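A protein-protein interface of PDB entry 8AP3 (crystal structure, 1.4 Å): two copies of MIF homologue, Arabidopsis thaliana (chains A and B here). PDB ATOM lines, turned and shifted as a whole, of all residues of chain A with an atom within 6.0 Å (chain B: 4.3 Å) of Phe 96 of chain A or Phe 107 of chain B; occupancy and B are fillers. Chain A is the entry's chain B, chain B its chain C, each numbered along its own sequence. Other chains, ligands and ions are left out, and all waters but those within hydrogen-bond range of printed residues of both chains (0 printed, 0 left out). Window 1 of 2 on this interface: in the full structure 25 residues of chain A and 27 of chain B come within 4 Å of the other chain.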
ATOM      1  N   LEU A   5     -14.128  -1.123  23.033  1.00  0.00           N
ATOM      2  CA  LEU A   5     -13.798  -0.737  21.665  1.00  0.00           C
ATOM      3  C   LEU A   5     -13.925   0.764  21.444  1.00  0.00           C
ATOM      4  O   LEU A   5     -14.847   1.425  21.952  1.00  0.00           O
ATOM      5  CB  LEU A   5     -14.736  -1.405  20.675  1.00  0.00           C
ATOM      6  CG  LEU A   5     -14.544  -2.913  20.573  1.00  0.00           C
ATOM      7  CD1 LEU A   5     -15.799  -3.535  20.010  1.00  0.00           C
ATOM      8  CD2 LEU A   5     -13.337  -3.257  19.703  1.00  0.00           C
ATOM      9  N   PHE A  50      -4.117   5.247  12.046  1.00  0.00           N
ATOM     10  CA  PHE A  50      -3.466   3.938  11.978  1.00  0.00           C
ATOM     11  C   PHE A  50      -2.571   3.973  10.756  1.00  0.00           C
ATOM     12  O   PHE A  50      -3.036   4.332   9.663  1.00  0.00           O
ATOM     13  CB  PHE A  50      -4.518   2.830  11.821  1.00  0.00           C
ATOM     14  CG  PHE A  50      -3.978   1.432  11.956  1.00  0.00           C
ATOM     15  CD1 PHE A  50      -3.207   0.855  10.951  1.00  0.00           C
ATOM     16  CD2 PHE A  50      -4.345   0.667  13.065  1.00  0.00           C
ATOM     17  CE1 PHE A  50      -2.723  -0.424  11.063  1.00  0.00           C
ATOM     18  CE2 PHE A  50      -3.863  -0.622  13.210  1.00  0.00           C
ATOM     19  CZ  PHE A  50      -3.031  -1.172  12.202  1.00  0.00           C
ATOM     20  N   ALA A  58     -10.078   0.803  14.240  1.00  0.00           N
ATOM     21  CA  ALA A  58     -10.635   0.577  15.563  1.00  0.00           C
ATOM     22  C   ALA A  58      -9.554   0.038  16.498  1.00  0.00           C
ATOM     23  O   ALA A  58      -8.595  -0.620  16.068  1.00  0.00           O
ATOM     24  CB  ALA A  58     -11.805  -0.415  15.503  1.00  0.00           C
ATOM     25  N   TYR A  59      -9.697   0.360  17.796  1.00  0.00           N
ATOM     26  CA  TYR A  59      -8.821  -0.178  18.832  1.00  0.00           C
ATOM     27  C   TYR A  59      -9.691  -0.825  19.896  1.00  0.00           C
ATOM     28  O   TYR A  59     -10.668  -0.217  20.349  1.00  0.00           O
ATOM     29  CB  TYR A  59      -7.971   0.929  19.475  1.00  0.00           C
ATOM     30  CG  TYR A  59      -7.064   0.390  20.547  1.00  0.00           C
ATOM     31  CD1 TYR A  59      -6.103  -0.596  20.251  1.00  0.00           C
ATOM     32  CD2 TYR A  59      -7.216   0.761  21.864  1.00  0.00           C
ATOM     33  CE1 TYR A  59      -5.292  -1.161  21.221  1.00  0.00           C
ATOM     34  CE2 TYR A  59      -6.388   0.199  22.852  1.00  0.00           C
ATOM     35  CZ  TYR A  59      -5.440  -0.753  22.520  1.00  0.00           C
ATOM     36  OH  TYR A  59      -4.656  -1.299  23.490  1.00  0.00           O
ATOM     37  N   GLY A  60      -9.353  -2.039  20.297  1.00  0.00           N
ATOM     38  CA  GLY A  60     -10.092  -2.723  21.335  1.00  0.00           C
ATOM     39  C   GLY A  60      -9.174  -3.310  22.387  1.00  0.00           C
ATOM     40  O   GLY A  60      -7.999  -3.563  22.140  1.00  0.00           O
ATOM     41  N   GLU A  61      -9.740  -3.541  23.571  1.00  0.00           N
ATOM     42  CA  GLU A  61      -9.094  -4.294  24.636  1.00  0.00           C
ATOM     43  C   GLU A  61     -10.100  -5.306  25.147  1.00  0.00           C
ATOM     44  O   GLU A  61     -11.269  -4.962  25.367  1.00  0.00           O
ATOM     45  CB  GLU A  61      -8.641  -3.356  25.757  1.00  0.00           C
ATOM     46  CG  GLU A  61      -7.552  -2.436  25.259  1.00  0.00           C
ATOM     47  CD  GLU A  61      -6.806  -1.684  26.344  1.00  0.00           C
ATOM     48  OE1 GLU A  61      -7.300  -1.649  27.495  1.00  0.00           O
ATOM     49  OE2 GLU A  61      -5.704  -1.133  26.030  1.00  0.00           O
ATOM     50  N   ASN A  73      -7.369 -16.328  21.538  1.00  0.00           N
ATOM     51  CA  ASN A  73      -7.186 -14.945  21.120  1.00  0.00           C
ATOM     52  C   ASN A  73      -7.313 -14.817  19.609  1.00  0.00           C
ATOM     53  O   ASN A  73      -7.879 -13.842  19.109  1.00  0.00           O
ATOM     54  CB  ASN A  73      -5.825 -14.425  21.594  1.00  0.00           C
ATOM     55  CG  ASN A  73      -5.693 -14.357  23.104  1.00  0.00           C
ATOM     56  OD1 ASN A  73      -6.646 -14.564  23.846  1.00  0.00           O
ATOM     57  ND2 ASN A  73      -4.482 -14.084  23.569  1.00  0.00           N
ATOM     58  N   LYS A  92     -10.029  -5.287   8.862  1.00  0.00           N
ATOM     59  CA  LYS A  92      -9.319  -5.975   9.932  1.00  0.00           C
ATOM     60  C   LYS A  92      -7.840  -5.574   9.993  1.00  0.00           C
ATOM     61  O   LYS A  92      -7.232  -5.618  11.067  1.00  0.00           O
ATOM     62  CB  LYS A  92      -9.490  -7.474   9.781  1.00  0.00           C
ATOM     63  CG  LYS A  92      -8.872  -8.035   8.522  1.00  0.00           C
ATOM     64  CD  LYS A  92      -9.272  -9.492   8.374  1.00  0.00           C
ATOM     65  CE  LYS A  92      -9.146  -9.964   6.938  1.00  0.00           C
ATOM     66  NZ  LYS A  92      -9.974  -9.089   6.036  1.00  0.00           N
ATOM     67  N   ARG A  94      -6.804  -2.704  10.024  1.00  0.00           N
ATOM     68  CA  ARG A  94      -6.785  -1.438  10.752  1.00  0.00           C
ATOM     69  C   ARG A  94      -7.452  -1.595  12.112  1.00  0.00           C
ATOM     70  O   ARG A  94      -7.984  -0.631  12.663  1.00  0.00           O
ATOM     71  CB  ARG A  94      -7.420  -0.312   9.925  1.00  0.00           C
ATOM     72  CG  ARG A  94      -6.655  -0.088   8.627  1.00  0.00           C
ATOM     73  CD  ARG A  94      -7.296   0.986   7.777  1.00  0.00           C
ATOM     74  NE  ARG A  94      -7.365   2.277   8.458  1.00  0.00           N
ATOM     75  CZ  ARG A  94      -6.339   3.113   8.600  1.00  0.00           C
ATOM     76  NH1 ARG A  94      -5.146   2.819   8.095  1.00  0.00           N
ATOM     77  NH2 ARG A  94      -6.512   4.267   9.244  1.00  0.00           N
ATOM     78  N   PHE A  95      -7.423  -2.804  12.666  1.00  0.00           N
ATOM     79  CA  PHE A  95      -8.044  -3.091  13.959  1.00  0.00           C
ATOM     80  C   PHE A  95      -7.002  -3.792  14.811  1.00  0.00           C
ATOM     81  O   PHE A  95      -6.558  -4.890  14.465  1.00  0.00           O
ATOM     82  CB  PHE A  95      -9.274  -3.993  13.756  1.00  0.00           C
ATOM     83  CG  PHE A  95      -9.919  -4.493  15.043  1.00  0.00           C
ATOM     84  CD1 PHE A  95      -9.938  -3.722  16.198  1.00  0.00           C
ATOM     85  CD2 PHE A  95     -10.485  -5.751  15.082  1.00  0.00           C
ATOM     86  CE1 PHE A  95     -10.554  -4.189  17.369  1.00  0.00           C
ATOM     87  CE2 PHE A  95     -11.058  -6.253  16.233  1.00  0.00           C
ATOM     88  CZ  PHE A  95     -11.113  -5.476  17.384  1.00  0.00           C
ATOM     89  N   PHE A  96      -6.606  -3.152  15.915  1.00  0.00           N
ATOM     90  CA  PHE A  96      -5.772  -3.767  16.941  1.00  0.00           C
ATOM     91  C   PHE A  96      -6.631  -4.137  18.152  1.00  0.00           C
ATOM     92  O   PHE A  96      -7.508  -3.365  18.569  1.00  0.00           O
ATOM     93  CB  PHE A  96      -4.746  -2.753  17.461  1.00  0.00           C
ATOM     94  CG  PHE A  96      -3.484  -2.613  16.623  1.00  0.00           C
ATOM     95  CD1 PHE A  96      -3.003  -3.616  15.787  1.00  0.00           C
ATOM     96  CD2 PHE A  96      -2.746  -1.459  16.770  1.00  0.00           C
ATOM     97  CE1 PHE A  96      -1.795  -3.430  15.083  1.00  0.00           C
ATOM     98  CE2 PHE A  96      -1.530  -1.274  16.092  1.00  0.00           C
ATOM     99  CZ  PHE A  96      -1.053  -2.265  15.261  1.00  0.00           C
ATOM    100  N   LEU A  97      -6.369  -5.296  18.745  1.00  0.00           N
ATOM    101  CA  LEU A  97      -7.172  -5.790  19.871  1.00  0.00           C
ATOM    102  C   LEU A  97      -6.221  -6.345  20.933  1.00  0.00           C
ATOM    103  O   LEU A  97      -5.638  -7.426  20.767  1.00  0.00           O
ATOM    104  CB  LEU A  97      -8.121  -6.885  19.389  1.00  0.00           C
ATOM    105  CG  LEU A  97      -9.009  -7.511  20.469  1.00  0.00           C
ATOM    106  CD1 LEU A  97      -9.789  -6.483  21.294  1.00  0.00           C
ATOM    107  CD2 LEU A  97      -9.977  -8.456  19.764  1.00  0.00           C
ATOM    108  N   LYS A  98      -6.041  -5.614  22.025  1.00  0.00           N
ATOM    109  CA  LYS A  98      -5.161  -6.058  23.092  1.00  0.00           C
ATOM    110  C   LYS A  98      -5.920  -6.987  24.030  1.00  0.00           C
ATOM    111  O   LYS A  98      -6.983  -6.623  24.524  1.00  0.00           O
ATOM    112  CB  LYS A  98      -4.655  -4.822  23.845  1.00  0.00           C
ATOM    113  CG  LYS A  98      -3.887  -5.098  25.150  1.00  0.00           C
ATOM    114  CD  LYS A  98      -2.722  -6.115  24.993  1.00  0.00           C
ATOM    115  CE  LYS A  98      -2.123  -6.499  26.345  1.00  0.00           C
ATOM    116  NZ  LYS A  98      -1.635  -7.883  26.239  1.00  0.00           N
ATOM    117  N   PHE A  99      -5.380  -8.161  24.303  1.00  0.00           N
ATOM    118  CA  PHE A  99      -5.978  -9.133  25.206  1.00  0.00           C
ATOM    119  C   PHE A  99      -5.263  -9.069  26.544  1.00  0.00           C
ATOM    120  O   PHE A  99      -4.027  -9.088  26.599  1.00  0.00           O
ATOM    121  CB  PHE A  99      -5.799 -10.551  24.613  1.00  0.00           C
ATOM    122  CG  PHE A  99      -6.582 -10.778  23.343  1.00  0.00           C
ATOM    123  CD1 PHE A  99      -6.010 -10.566  22.100  1.00  0.00           C
ATOM    124  CD2 PHE A  99      -7.923 -11.157  23.410  1.00  0.00           C
ATOM    125  CE1 PHE A  99      -6.742 -10.761  20.935  1.00  0.00           C
ATOM    126  CE2 PHE A  99      -8.656 -11.349  22.245  1.00  0.00           C
ATOM    127  CZ  PHE A  99      -8.083 -11.150  21.019  1.00  0.00           C
ATOM    128  N   PRO B   1       2.399  -0.559  17.715  1.00  0.00           N
ATOM    129  CA  PRO B   1       1.964  -0.106  19.042  1.00  0.00           C
ATOM    130  C   PRO B   1       0.742   0.753  18.954  1.00  0.00           C
ATOM    131  O   PRO B   1       0.408   1.212  17.883  1.00  0.00           O
ATOM    132  CB  PRO B   1       3.124   0.748  19.542  1.00  0.00           C
ATOM    133  CG  PRO B   1       3.917   1.086  18.351  1.00  0.00           C
ATOM    134  CD  PRO B   1       3.693   0.028  17.315  1.00  0.00           C
ATOM    135  N   TYR B  37       2.504   0.230  11.598  1.00  0.00           N
ATOM    136  CA  TYR B  37       1.962  -0.492  12.737  1.00  0.00           C
ATOM    137  C   TYR B  37       1.677   0.410  13.925  1.00  0.00           C
ATOM    138  O   TYR B  37       1.459  -0.102  15.026  1.00  0.00           O
ATOM    139  CB  TYR B  37       2.911  -1.617  13.158  1.00  0.00           C
ATOM    140  CG  TYR B  37       2.916  -2.811  12.232  1.00  0.00           C
ATOM    141  CD1 TYR B  37       2.050  -3.875  12.430  1.00  0.00           C
ATOM    142  CD2 TYR B  37       3.785  -2.862  11.158  1.00  0.00           C
ATOM    143  CE1 TYR B  37       2.048  -4.971  11.589  1.00  0.00           C
ATOM    144  CE2 TYR B  37       3.798  -3.977  10.298  1.00  0.00           C
ATOM    145  CZ  TYR B  37       2.925  -5.017  10.520  1.00  0.00           C
ATOM    146  OH  TYR B  37       2.902  -6.125   9.690  1.00  0.00           O
ATOM    147  N   MET B  39      -0.714   3.010  15.896  1.00  0.00           N
ATOM    148  CA  MET B  39      -2.068   3.517  16.055  1.00  0.00           C
ATOM    149  C   MET B  39      -2.048   4.590  17.138  1.00  0.00           C
ATOM    150  O   MET B  39      -1.439   4.400  18.196  1.00  0.00           O
ATOM    151  CB  MET B  39      -2.985   2.358  16.455  1.00  0.00           C
ATOM    152  CG  MET B  39      -4.434   2.798  16.657  1.00  0.00           C
ATOM    153  SD  MET B  39      -5.542   1.353  16.659  1.00  0.00           S
ATOM    154  CE  MET B  39      -6.985   2.113  15.912  1.00  0.00           C
ATOM    155  N   VAL B  63       0.655   0.654  24.422  1.00  0.00           N
ATOM    156  CA  VAL B  63       0.914  -0.785  24.358  1.00  0.00           C
ATOM    157  C   VAL B  63       1.803  -1.047  23.147  1.00  0.00           C
ATOM    158  O   VAL B  63       1.567  -0.497  22.070  1.00  0.00           O
ATOM    159  CB  VAL B  63      -0.420  -1.548  24.216  1.00  0.00           C
ATOM    160  CG1 VAL B  63      -0.194  -3.018  24.151  1.00  0.00           C
ATOM    161  CG2 VAL B  63      -1.426  -1.174  25.335  1.00  0.00           C
ATOM    162  N   ILE B  65       4.275  -4.376  21.152  1.00  0.00           N
ATOM    163  CA  ILE B  65       4.895  -5.705  21.155  1.00  0.00           C
ATOM    164  C   ILE B  65       6.399  -5.502  21.272  1.00  0.00           C
ATOM    165  O   ILE B  65       7.086  -5.266  20.258  1.00  0.00           O
ATOM    166  CB  ILE B  65       4.539  -6.498  19.887  1.00  0.00           C
ATOM    167  CG1 ILE B  65       3.014  -6.570  19.716  1.00  0.00           C
ATOM    168  CG2 ILE B  65       5.168  -7.881  19.942  1.00  0.00           C
ATOM    169  CD1 ILE B  65       2.634  -7.221  18.389  1.00  0.00           C
ATOM    170  N   THR B 102       3.309  -6.075  25.491  1.00  0.00           N
ATOM    171  CA  THR B 102       2.479  -7.248  25.243  1.00  0.00           C
ATOM    172  C   THR B 102       3.200  -8.295  24.402  1.00  0.00           C
ATOM    173  O   THR B 102       3.999  -7.964  23.504  1.00  0.00           O
ATOM    174  CB  THR B 102       1.181  -6.827  24.531  1.00  0.00           C
ATOM    175  OG1 THR B 102       0.330  -7.973  24.368  1.00  0.00           O
ATOM    176  CG2 THR B 102       1.447  -6.228  23.178  1.00  0.00           C
ATOM    177  N   LYS B 103       2.880  -9.559  24.671  1.00  0.00           N
ATOM    178  CA  LYS B 103       3.232 -10.623  23.735  1.00  0.00           C
ATOM    179  C   LYS B 103       2.408 -10.458  22.475  1.00  0.00           C
ATOM    180  O   LYS B 103       1.240 -10.036  22.529  1.00  0.00           O
ATOM    181  CB  LYS B 103       2.858 -11.981  24.337  1.00  0.00           C
ATOM    182  CG  LYS B 103       3.697 -12.411  25.533  1.00  0.00           C
ATOM    183  CD  LYS B 103       3.100 -13.660  26.221  1.00  0.00           C
ATOM    184  CE  LYS B 103       4.143 -14.375  27.055  1.00  0.00           C
ATOM    185  NZ  LYS B 103       3.521 -15.362  27.985  1.00  0.00           N
ATOM    186  N   GLY B 104       2.993 -10.783  21.317  1.00  0.00           N
ATOM    187  CA  GLY B 104       2.216 -10.748  20.094  1.00  0.00           C
ATOM    188  C   GLY B 104       0.987 -11.639  20.116  1.00  0.00           C
ATOM    189  O   GLY B 104      -0.033 -11.312  19.503  1.00  0.00           O
ATOM    190  N   SER B 105       1.082 -12.789  20.775  1.00  0.00           N
ATOM    191  CA  SER B 105      -0.073 -13.681  20.815  1.00  0.00           C
ATOM    192  C   SER B 105      -1.225 -13.110  21.621  1.00  0.00           C
ATOM    193  O   SER B 105      -2.333 -13.670  21.590  1.00  0.00           O
ATOM    194  CB  SER B 105       0.333 -15.006  21.419  1.00  0.00           C
ATOM    195  OG  SER B 105       0.790 -14.798  22.721  1.00  0.00           O
ATOM    196  N   PHE B 106      -0.981 -12.038  22.369  1.00  0.00           N
ATOM    197  CA  PHE B 106      -2.034 -11.325  23.075  1.00  0.00           C
ATOM    198  C   PHE B 106      -2.344  -9.986  22.425  1.00  0.00           C
ATOM    199  O   PHE B 106      -2.894  -9.076  23.076  1.00  0.00           O
ATOM    200  CB  PHE B 106      -1.696 -11.193  24.561  1.00  0.00           C
ATOM    201  CG  PHE B 106      -2.014 -12.429  25.352  1.00  0.00           C
ATOM    202  CD1 PHE B 106      -1.410 -13.655  25.077  1.00  0.00           C
ATOM    203  CD2 PHE B 106      -2.993 -12.366  26.352  1.00  0.00           C
ATOM    204  CE1 PHE B 106      -1.745 -14.785  25.816  1.00  0.00           C
ATOM    205  CE2 PHE B 106      -3.334 -13.498  27.089  1.00  0.00           C
ATOM    206  CZ  PHE B 106      -2.700 -14.713  26.812  1.00  0.00           C
ATOM    207  N   PHE B 107      -2.069  -9.849  21.127  1.00  0.00           N
ATOM    208  CA  PHE B 107      -2.326  -8.615  20.395  1.00  0.00           C
ATOM    209  C   PHE B 107      -2.942  -8.978  19.051  1.00  0.00           C
ATOM    210  O   PHE B 107      -2.272  -9.509  18.155  1.00  0.00           O
ATOM    211  CB  PHE B 107      -1.059  -7.765  20.252  1.00  0.00           C
ATOM    212  CG  PHE B 107      -1.330  -6.296  20.077  1.00  0.00           C
ATOM    213  CD1 PHE B 107      -1.824  -5.544  21.126  1.00  0.00           C
ATOM    214  CD2 PHE B 107      -1.058  -5.649  18.891  1.00  0.00           C
ATOM    215  CE1 PHE B 107      -2.062  -4.194  20.982  1.00  0.00           C
ATOM    216  CE2 PHE B 107      -1.289  -4.263  18.742  1.00  0.00           C
ATOM    217  CZ  PHE B 107      -1.787  -3.553  19.789  1.00  0.00           C
ATOM    218  N   GLY B 108      -4.236  -8.743  18.927  1.00  0.00           N
ATOM    219  CA  GLY B 108      -4.928  -9.057  17.683  1.00  0.00           C
ATOM    220  C   GLY B 108      -4.685  -7.988  16.629  1.00  0.00           C
ATOM    221  O   GLY B 108      -4.648  -6.782  16.913  1.00  0.00           O
ATOM    222  N   TRP B 109      -4.522  -8.447  15.382  1.00  0.00           N
ATOM    223  CA  TRP B 109      -4.418  -7.558  14.236  1.00  0.00           C
ATOM    224  C   TRP B 109      -4.736  -8.386  13.000  1.00  0.00           C
ATOM    225  O   TRP B 109      -4.411  -9.575  12.957  1.00  0.00           O
ATOM    226  CB  TRP B 109      -2.995  -6.985  14.107  1.00  0.00           C
ATOM    227  CG  TRP B 109      -2.845  -6.199  12.839  1.00  0.00           C
ATOM    228  CD1 TRP B 109      -3.462  -5.023  12.539  1.00  0.00           C
ATOM    229  CD2 TRP B 109      -2.088  -6.561  11.664  1.00  0.00           C
ATOM    230  NE1 TRP B 109      -3.127  -4.601  11.266  1.00  0.00           N
ATOM    231  CE2 TRP B 109      -2.283  -5.535  10.715  1.00  0.00           C
ATOM    232  CE3 TRP B 109      -1.250  -7.641  11.337  1.00  0.00           C
ATOM    233  CZ2 TRP B 109      -1.680  -5.564   9.449  1.00  0.00           C
ATOM    234  CZ3 TRP B 109      -0.667  -7.663  10.065  1.00  0.00           C
ATOM    235  CH2 TRP B 109      -0.883  -6.626   9.155  1.00  0.00           C
ATOM    236  N   THR B 113      -3.668 -12.983  15.354  1.00  0.00           N
ATOM    237  CA  THR B 113      -2.810 -12.307  16.313  1.00  0.00           C
ATOM    238  C   THR B 113      -1.453 -12.067  15.683  1.00  0.00           C
ATOM    239  O   THR B 113      -1.162 -12.508  14.569  1.00  0.00           O
ATOM    240  CB  THR B 113      -2.641 -13.088  17.607  1.00  0.00           C
ATOM    241  OG1 THR B 113      -1.835 -14.250  17.367  1.00  0.00           O
ATOM    242  CG2 THR B 113      -3.988 -13.500  18.169  1.00  0.00           C
ATOM    243  N   LEU B 114      -0.614 -11.343  16.412  1.00  0.00           N
ATOM    244  CA  LEU B 114       0.759 -11.110  15.986  1.00  0.00           C
ATOM    245  C   LEU B 114       1.692 -12.049  16.718  1.00  0.00           C
ATOM    246  O   LEU B 114       2.786 -11.685  17.150  1.00  0.00           O
ATOM    247  CB  LEU B 114       1.137  -9.633  16.144  1.00  0.00           C
ATOM    248  CG  LEU B 114       0.560  -8.807  14.981  1.00  0.00           C
ATOM    249  CD1 LEU B 114       0.666  -7.308  15.230  1.00  0.00           C
ATOM    250  CD2 LEU B 114       1.276  -9.165  13.681  1.00  0.00           C
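Of the printed residues of chain B, Phe 50 of chain A touches Met 39 (3.8 Å) and Trp 109 (3.6 Å).
Glu 61 of chain A touches none of the printed residues of chain B.
Phe 96 of chain A touches just these residues of chain B: Pro 1 (3.6 Å), Tyr 37 (3.3 Å), Met 39 (3.8 Å), Phe 107 (3.5 Å), Gly 108 (3.2 Å) and Trp 109 (3.4 Å).
Of the printed residues of chain B, Leu 97 of chain A touches Phe 106, Phe 107 and Gly 108.
Phe 107 of chain B touches three residues of chain A.
Of the printed residues of chain A, Thr 113 of chain B touches Asn 73 (3.9 Å).
The nearest printed residue of chain B that does not touch Phe 96 of chain A is Leu 114 of chain B (4.6 Å).
The nearest printed residue of chain A that does not touch Thr 102 of chain B is Phe 99 of chain A (5.0 Å).
No position is printed for both chains.
Of the 24 pairs that touch across the chains among the printed residues, none has its exchanged pair printed and touching as well.
The backbone carbonyl oxygen of Ala 58 of chain A sits at hydrogen-bond distance from the backbone NH of Phe 96 of chain A.
O of Pro 1 of chain B is in hydrogen-bond range of N of Met 39 of chain B (2.9 Å).
The guanidinium group (NH1) of Arg 94 of chain A lies within hydrogen-bond range of the backbone carbonyl oxygen (O) of Phe 50 of chain A (3.0 Å).
The side-chain hydroxyl (OH) of Tyr 59 of chain A lies within hydrogen-bond range of the side-chain carboxylate (OE2) of Glu 61 of chain A (2.8 Å).
The backbone NH (N) of Ala 58 of chain A sits at hydrogen-bond distance from the backbone carbonyl oxygen (O) of Arg 94 of chain A, 3.0 Å away.
The backbone carbonyl oxygen (O) of Gly 60 of chain A is in hydrogen-bond range of the backbone NH (N) of Lys 98 of chain A, at 2.8 Å.
N of Gly 108 of chain B is in hydrogen-bond range of O of Leu 97 of chain A.
The side-chain amino group (NZ) of Lys 98 of chain A sits at hydrogen-bond distance from the side-chain hydroxyl (OG1) of Thr 102 of chain B.
The backbone carbonyl oxygen of Ser 105 of chain B sits at hydrogen-bond distance from the side-chain amide nitrogen of Asn 73 of chain A (3.0 Å).
The backbone NH (N) of Phe 99 of chain A lies within hydrogen-bond range of the backbone carbonyl oxygen (O) of Phe 106 of chain B (2.9 Å).
O of Ala 58 of chain A sits close to SD of Met 39 of chain B, at 3.7 Å.
Of the 15 printed residues of chain B, 11 touch a printed residue of chain A.
Printed residues of chain B that touch a printed residue of chain A: Pro 1, Tyr 37, Met 39, Val 63, Thr 102, Ser 105, Phe 106, Phe 107, Gly 108, Trp 109 and Thr 113.
Along chain B the printed residues that touch a printed residue of chain A span positions 1 to 113.
Of the 14 printed residues of chain A, 9 touch a printed residue of chain B.
Printed residues of chain A that touch a printed residue of chain B: Phe 50, Ala 58, Tyr 59, Asn 73, Phe 95, Phe 96, Leu 97, Lys 98 and Phe 99.
Among the printed residues, pairs that only touch across the chains: Phe 96 of chain A with Gly 108 of chain B (3.2 Å), Phe 96 of chain A with Tyr 37 of chain B (3.3 Å), Phe 95 of chain A with Trp 109 of chain B (3.4 Å), Phe 96 of chain A with Trp 109 of chain B (3.4 Å), Asn 73 of chain A with Phe 106 of chain B (3.4 Å), Phe 96 of chain A with Phe 107 of chain B (3.5 Å), Lys 98 of chain A with Phe 106 of chain B (3.5 Å), Leu 97 of chain A with Phe 107 of chain B (3.5 Å), Phe 50 of chain A with Trp 109 of chain B (3.6 Å), Phe 96 of chain A with Pro 1 of chain B (3.6 Å), Phe 95 of chain A with Gly 108 of chain B (3.6 Å), Tyr 59 of chain A with Val 63 of chain B (3.7 Å), Tyr 59 of chain A with Met 39 of chain B (3.7 Å), Phe 99 of chain A with Gly 108 of chain B (3.8 Å), Phe 96 of chain A with Met 39 of chain B (3.8 Å), Phe 50 of chain A with Met 39 of chain B (3.8 Å), Asn 73 of chain A with Thr 113 of chain B (3.9 Å), Lys 98 of chain A with Phe 107 of chain B (3.9 Å) and Leu 97 of chain A with Phe 106 of chain B (3.9 Å).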
